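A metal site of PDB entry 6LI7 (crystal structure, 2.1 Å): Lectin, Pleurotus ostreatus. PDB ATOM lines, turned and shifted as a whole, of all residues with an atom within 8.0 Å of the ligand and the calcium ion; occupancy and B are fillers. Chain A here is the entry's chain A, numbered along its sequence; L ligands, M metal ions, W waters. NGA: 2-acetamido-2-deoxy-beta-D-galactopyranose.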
ATOM      1  N   TRP A 222     -21.175  37.613  29.235  1.00  0.00           N
ATOM      2  CA  TRP A 222     -21.915  37.193  28.031  1.00  0.00           C
ATOM      3  C   TRP A 222     -22.689  38.413  27.491  1.00  0.00           C
ATOM      4  O   TRP A 222     -22.644  39.534  28.085  1.00  0.00           O
ATOM      5  CB  TRP A 222     -22.831  35.996  28.391  1.00  0.00           C
ATOM      6  CG  TRP A 222     -23.159  35.073  27.263  1.00  0.00           C
ATOM      7  CD1 TRP A 222     -24.371  34.960  26.667  1.00  0.00           C
ATOM      8  CD2 TRP A 222     -22.282  34.167  26.579  1.00  0.00           C
ATOM      9  NE1 TRP A 222     -24.309  34.042  25.677  1.00  0.00           N
ATOM     10  CE2 TRP A 222     -23.035  33.536  25.581  1.00  0.00           C
ATOM     11  CE3 TRP A 222     -20.933  33.810  26.706  1.00  0.00           C
ATOM     12  CZ2 TRP A 222     -22.513  32.576  24.723  1.00  0.00           C
ATOM     13  CZ3 TRP A 222     -20.406  32.871  25.842  1.00  0.00           C
ATOM     14  CH2 TRP A 222     -21.197  32.237  24.881  1.00  0.00           C
ATOM     15  N   GLY A 229     -29.756  32.062  34.686  1.00  0.00           N
ATOM     16  CA  GLY A 229     -28.764  30.966  34.758  1.00  0.00           C
ATOM     17  C   GLY A 229     -28.615  30.188  33.459  1.00  0.00           C
ATOM     18  O   GLY A 229     -28.024  29.095  33.472  1.00  0.00           O
ATOM     19  N   ALA A 230     -29.136  30.702  32.357  1.00  0.00           N
ATOM     20  CA  ALA A 230     -29.003  30.023  31.054  1.00  0.00           C
ATOM     21  C   ALA A 230     -28.992  31.090  29.966  1.00  0.00           C
ATOM     22  O   ALA A 230     -29.415  32.253  30.210  1.00  0.00           O
ATOM     23  CB  ALA A 230     -30.102  29.010  30.853  1.00  0.00           C
ATOM     24  N   ALA A 231     -28.462  30.729  28.818  1.00  0.00           N
ATOM     25  CA  ALA A 231     -28.497  31.642  27.650  1.00  0.00           C
ATOM     26  C   ALA A 231     -28.890  30.802  26.475  1.00  0.00           C
ATOM     27  O   ALA A 231     -28.675  29.595  26.522  1.00  0.00           O
ATOM     28  CB  ALA A 231     -27.138  32.245  27.407  1.00  0.00           C
ATOM     29  N   PRO A 232     -29.340  31.433  25.373  1.00  0.00           N
ATOM     30  CA  PRO A 232     -29.702  30.689  24.175  1.00  0.00           C
ATOM     31  C   PRO A 232     -28.504  29.946  23.600  1.00  0.00           C
ATOM     32  O   PRO A 232     -27.341  30.312  23.864  1.00  0.00           O
ATOM     33  CB  PRO A 232     -30.244  31.763  23.210  1.00  0.00           C
ATOM     34  CG  PRO A 232     -30.604  32.925  24.101  1.00  0.00           C
ATOM     35  CD  PRO A 232     -29.661  32.869  25.284  1.00  0.00           C
ATOM     36  N   VAL A 233     -28.817  28.874  22.862  1.00  0.00           N
ATOM     37  CA  VAL A 233     -27.825  28.156  22.025  1.00  0.00           C
ATOM     38  C   VAL A 233     -27.380  29.159  20.951  1.00  0.00           C
ATOM     39  O   VAL A 233     -28.216  29.914  20.495  1.00  0.00           O
ATOM     40  CB  VAL A 233     -28.402  26.874  21.418  1.00  0.00           C
ATOM     41  CG1 VAL A 233     -27.396  26.218  20.484  1.00  0.00           C
ATOM     42  CG2 VAL A 233     -28.829  25.888  22.514  1.00  0.00           C
ATOM     43  N   ALA A 258     -14.100  29.231  28.155  1.00  0.00           N
ATOM     44  CA  ALA A 258     -15.496  29.552  27.835  1.00  0.00           C
ATOM     45  C   ALA A 258     -16.416  28.345  28.056  1.00  0.00           C
ATOM     46  O   ALA A 258     -16.057  27.227  27.706  1.00  0.00           O
ATOM     47  CB  ALA A 258     -15.576  30.048  26.403  1.00  0.00           C
ATOM     48  N   ASP A 259     -17.636  28.641  28.484  1.00  0.00           N
ATOM     49  CA  ASP A 259     -18.776  27.717  28.468  1.00  0.00           C
ATOM     50  C   ASP A 259     -19.655  27.983  27.223  1.00  0.00           C
ATOM     51  O   ASP A 259     -20.298  29.031  27.252  1.00  0.00           O
ATOM     52  CB  ASP A 259     -19.602  27.868  29.727  1.00  0.00           C
ATOM     53  CG  ASP A 259     -20.799  26.931  29.780  1.00  0.00           C
ATOM     54  OD1 ASP A 259     -21.134  26.328  28.738  1.00  0.00           O
ATOM     55  OD2 ASP A 259     -21.341  26.778  30.881  1.00  0.00           O
ATOM     56  N   ASP A 260     -19.241  27.399  26.116  1.00  0.00           N
ATOM     57  CA  ASP A 260     -18.949  25.964  25.885  1.00  0.00           C
ATOM     58  C   ASP A 260     -17.615  25.938  25.152  1.00  0.00           C
ATOM     59  O   ASP A 260     -16.830  25.004  25.360  1.00  0.00           O
ATOM     60  CB  ASP A 260     -20.071  25.214  25.162  1.00  0.00           C
ATOM     61  CG  ASP A 260     -21.087  24.668  26.135  1.00  0.00           C
ATOM     62  OD1 ASP A 260     -20.692  23.752  26.893  1.00  0.00           O
ATOM     63  OD2 ASP A 260     -22.218  25.234  26.225  1.00  0.00           O
ATOM     64  N   ARG A 261     -17.308  26.982  24.357  1.00  0.00           N
ATOM     65  CA  ARG A 261     -16.139  26.960  23.448  1.00  0.00           C
ATOM     66  C   ARG A 261     -15.852  28.392  22.960  1.00  0.00           C
ATOM     67  O   ARG A 261     -16.705  29.266  23.157  1.00  0.00           O
ATOM     68  CB  ARG A 261     -16.402  26.003  22.279  1.00  0.00           C
ATOM     69  CG  ARG A 261     -17.485  26.473  21.314  1.00  0.00           C
ATOM     70  CD  ARG A 261     -18.022  25.451  20.304  1.00  0.00           C
ATOM     71  NE  ARG A 261     -17.004  24.487  19.951  1.00  0.00           N
ATOM     72  CZ  ARG A 261     -17.013  23.197  20.316  1.00  0.00           C
ATOM     73  NH1 ARG A 261     -18.026  22.706  21.011  1.00  0.00           N
ATOM     74  NH2 ARG A 261     -15.985  22.414  19.996  1.00  0.00           N
ATOM     75  N   TYR A 277     -14.725  24.534  29.876  1.00  0.00           N
ATOM     76  CA  TYR A 277     -14.988  25.494  30.949  1.00  0.00           C
ATOM     77  C   TYR A 277     -14.370  24.975  32.245  1.00  0.00           C
ATOM     78  O   TYR A 277     -14.544  25.664  33.231  1.00  0.00           O
ATOM     79  CB  TYR A 277     -16.467  25.803  31.039  1.00  0.00           C
ATOM     80  CG  TYR A 277     -17.401  24.621  31.161  1.00  0.00           C
ATOM     81  CD1 TYR A 277     -17.687  24.085  32.397  1.00  0.00           C
ATOM     82  CD2 TYR A 277     -18.069  24.136  30.052  1.00  0.00           C
ATOM     83  CE1 TYR A 277     -18.570  23.028  32.526  1.00  0.00           C
ATOM     84  CE2 TYR A 277     -18.950  23.076  30.158  1.00  0.00           C
ATOM     85  CZ  TYR A 277     -19.195  22.519  31.405  1.00  0.00           C
ATOM     86  OH  TYR A 277     -20.073  21.496  31.556  1.00  0.00           O
ATOM     87  N   THR A 300     -19.252  30.264  21.909  1.00  0.00           N
ATOM     88  CA  THR A 300     -20.479  29.537  21.509  1.00  0.00           C
ATOM     89  C   THR A 300     -21.063  28.815  22.731  1.00  0.00           C
ATOM     90  O   THR A 300     -20.321  28.100  23.392  1.00  0.00           O
ATOM     91  CB  THR A 300     -20.136  28.591  20.345  1.00  0.00           C
ATOM     92  OG1 THR A 300     -19.574  29.325  19.251  1.00  0.00           O
ATOM     93  CG2 THR A 300     -21.344  27.816  19.871  1.00  0.00           C
ATOM     94  N   ASN A 301     -22.359  28.997  22.973  1.00  0.00           N
ATOM     95  CA  ASN A 301     -23.169  28.214  23.937  1.00  0.00           C
ATOM     96  C   ASN A 301     -23.858  27.036  23.209  1.00  0.00           C
ATOM     97  O   ASN A 301     -24.639  27.242  22.269  1.00  0.00           O
ATOM     98  CB  ASN A 301     -24.167  29.094  24.686  1.00  0.00           C
ATOM     99  CG  ASN A 301     -24.854  28.295  25.802  1.00  0.00           C
ATOM    100  OD1 ASN A 301     -24.276  27.311  26.248  1.00  0.00           O
ATOM    101  ND2 ASN A 301     -26.069  28.668  26.189  1.00  0.00           N
ATOM    102  N   GLY A 302     -23.533  25.822  23.632  1.00  0.00           N
ATOM    103  CA  GLY A 302     -24.151  24.564  23.191  1.00  0.00           C
ATOM    104  C   GLY A 302     -25.467  24.285  23.918  1.00  0.00           C
ATOM    105  O   GLY A 302     -26.149  23.341  23.533  1.00  0.00           O
ATOM    106  N   GLY A 303     -25.784  25.054  24.956  1.00  0.00           N
ATOM    107  CA  GLY A 303     -26.942  24.795  25.824  1.00  0.00           C
ATOM    108  C   GLY A 303     -26.657  25.146  27.272  1.00  0.00           C
ATOM    109  O   GLY A 303     -25.509  24.997  27.710  1.00  0.00           O
ATOM    110  N   GLY A 304     -27.698  25.567  27.974  1.00  0.00           N
ATOM    111  CA  GLY A 304     -27.698  25.909  29.397  1.00  0.00           C
ATOM    112  C   GLY A 304     -26.876  27.161  29.646  1.00  0.00           C
ATOM    113  O   GLY A 304     -26.922  28.100  28.841  1.00  0.00           O
ATOM    114  N   PRO A 305     -26.185  27.195  30.813  1.00  0.00           N
ATOM    115  CA  PRO A 305     -25.383  28.350  31.213  1.00  0.00           C
ATOM    116  C   PRO A 305     -24.340  28.626  30.113  1.00  0.00           C
ATOM    117  O   PRO A 305     -23.962  27.685  29.308  1.00  0.00           O
ATOM    118  CB  PRO A 305     -24.706  27.932  32.551  1.00  0.00           C
ATOM    119  CG  PRO A 305     -25.634  26.833  33.115  1.00  0.00           C
ATOM    120  CD  PRO A 305     -26.160  26.140  31.861  1.00  0.00           C
ATOM    121  N   ALA A 306     -23.863  29.864  30.097  1.00  0.00           N
ATOM    122  CA  ALA A 306     -22.821  30.305  29.149  1.00  0.00           C
ATOM    123  C   ALA A 306     -22.001  31.424  29.781  1.00  0.00           C
ATOM    124  O   ALA A 306     -22.559  32.225  30.579  1.00  0.00           O
ATOM    125  CB  ALA A 306     -23.471  30.756  27.859  1.00  0.00           C
ATOM    126  N   GLY A 307     -20.754  31.524  29.342  1.00  0.00           N
ATOM    127  CA  GLY A 307     -19.878  32.619  29.791  1.00  0.00           C
ATOM    128  C   GLY A 307     -18.516  32.501  29.167  1.00  0.00           C
ATOM    129  O   GLY A 307     -18.101  31.394  28.747  1.00  0.00           O
ATOM    130  N   ALA A 362     -21.018  29.867  41.026  1.00  0.00           N
ATOM    131  CA  ALA A 362     -21.782  28.760  40.401  1.00  0.00           C
ATOM    132  C   ALA A 362     -22.235  29.195  39.002  1.00  0.00           C
ATOM    133  O   ALA A 362     -22.583  30.339  38.780  1.00  0.00           O
ATOM    134  CB  ALA A 362     -23.016  28.459  41.232  1.00  0.00           C
ATOM    135  N   PRO A 363     -22.381  28.301  38.047  1.00  0.00           N
ATOM    136  CA  PRO A 363     -22.140  26.887  38.262  1.00  0.00           C
ATOM    137  C   PRO A 363     -20.689  26.440  38.114  1.00  0.00           C
ATOM    138  O   PRO A 363     -20.408  25.313  38.338  1.00  0.00           O
ATOM    139  CB  PRO A 363     -22.941  26.243  37.099  1.00  0.00           C
ATOM    140  CG  PRO A 363     -22.817  27.292  36.013  1.00  0.00           C
ATOM    141  CD  PRO A 363     -22.972  28.608  36.743  1.00  0.00           C
ATOM    142  N   TRP A 364     -19.809  27.301  37.612  1.00  0.00           N
ATOM    143  CA  TRP A 364     -18.463  26.830  37.215  1.00  0.00           C
ATOM    144  C   TRP A 364     -17.586  26.720  38.481  1.00  0.00           C
ATOM    145  O   TRP A 364     -16.735  25.922  38.456  1.00  0.00           O
ATOM    146  CB  TRP A 364     -17.842  27.770  36.172  1.00  0.00           C
ATOM    147  CG  TRP A 364     -18.804  28.035  35.038  1.00  0.00           C
ATOM    148  CD1 TRP A 364     -19.115  27.182  34.020  1.00  0.00           C
ATOM    149  CD2 TRP A 364     -19.589  29.206  34.833  1.00  0.00           C
ATOM    150  NE1 TRP A 364     -20.034  27.776  33.193  1.00  0.00           N
ATOM    151  CE2 TRP A 364     -20.336  29.005  33.660  1.00  0.00           C
ATOM    152  CE3 TRP A 364     -19.703  30.429  35.501  1.00  0.00           C
ATOM    153  CZ2 TRP A 364     -21.218  29.972  33.165  1.00  0.00           C
ATOM    154  CZ3 TRP A 364     -20.565  31.389  35.000  1.00  0.00           C
ATOM    155  CH2 TRP A 364     -21.314  31.169  33.843  1.00  0.00           C
ATOM    156  N   GLY A 365     -17.742  27.530  39.499  1.00  0.00           N
ATOM    157  CA  GLY A 365     -16.896  27.364  40.702  1.00  0.00           C
ATOM    158  C   GLY A 365     -15.499  27.944  40.537  1.00  0.00           C
ATOM    159  O   GLY A 365     -15.206  28.571  39.498  1.00  0.00           O
HETATM  160  C1  NGA L   1     -24.363  21.884  31.281  1.00  0.00           C
HETATM  161  C2  NGA L   1     -24.369  22.445  29.838  1.00  0.00           C
HETATM  162  C3  NGA L   1     -22.930  22.907  29.505  1.00  0.00           C
HETATM  163  C4  NGA L   1     -22.488  23.853  30.626  1.00  0.00           C
HETATM  164  C5  NGA L   1     -22.798  23.340  32.066  1.00  0.00           C
HETATM  165  C6  NGA L   1     -22.363  24.364  33.095  1.00  0.00           C
HETATM  166  C7  NGA L   1     -26.181  21.615  28.366  1.00  0.00           C
HETATM  167  C8  NGA L   1     -26.536  20.577  27.340  1.00  0.00           C
HETATM  168  N2  NGA L   1     -24.953  21.481  28.867  1.00  0.00           N
HETATM  169  O1  NGA L   1     -25.565  21.294  31.612  1.00  0.00           O
HETATM  170  O3  NGA L   1     -22.829  23.637  28.235  1.00  0.00           O
HETATM  171  O4  NGA L   1     -23.185  25.140  30.382  1.00  0.00           O
HETATM  172  O5  NGA L   1     -24.221  23.033  32.159  1.00  0.00           O
HETATM  173  O6  NGA L   1     -22.546  23.931  34.399  1.00  0.00           O
HETATM  174  O7  NGA L   1     -27.025  22.497  28.688  1.00  0.00           O
HETATM  175 CA    CA M   1     -23.349  25.922  28.095  1.00  0.00          CA
HETATM  176  O   HOH W   1     -23.689  22.064  25.726  1.00  0.00           O
HETATM  177  O   HOH W   2     -26.806  21.583  34.033  1.00  0.00           O
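O7 of the ligand is in hydrogen-bond range of N of Gly 304 (3.2 Å).
Along chain A the residues within 4 Å of the calcium ion span positions 259 to 305.
OD2 of Asp 260 sits close to N of Gly 302 (3.0 Å).
The backbone carbonyl oxygen (O) of Thr 300 sits at hydrogen-bond distance from the backbone NH (N) of Asp 260 (3.0 Å).
NE1 of Trp 364 sits at hydrogen-bond distance from OD2 of Asp 259 (2.8 Å).
O of Gly 307 lies within hydrogen-bond range of N of Asp 259, at 2.8 Å.
O of Gly 304 sits at hydrogen-bond distance from ND2 of Asn 301, 2.8 Å away.
The side-chain amide nitrogen of Asn 301 lies within hydrogen-bond range of the backbone carbonyl oxygen of Ala 231 (2.8 Å).
The side-chain amide nitrogen (ND2) of Asn 301 sits at hydrogen-bond distance from the backbone carbonyl oxygen (O) of Pro 232.
O of Gly 304 sits at hydrogen-bond distance from N of Ala 231, 3.0 Å away.
OH of Tyr 277 touches C5 of the ligand (3.3 Å).
Pro 363 touches the ligand.
Hydrophobic or aromatic side chains within 4 Å of the ligand: Tyr 277, Pro 305 and Pro 363.
The calcium ion is bound by the backbone carbonyl oxygen (O) of Pro 305 (2.2 Å), the side-chain carboxylate (OD2) of Asp 260 (2.3 Å), the side-chain carboxylate (OD1) of Asp 259 (2.3 Å), an oxygen (O3) of the ligand (2.3 Å), the backbone carbonyl oxygen (O) of Gly 303 (2.4 Å), an oxygen (O4) of the ligand (2.4 Å) and the side-chain amide oxygen (OD1) of Asn 301 (2.5 Å).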
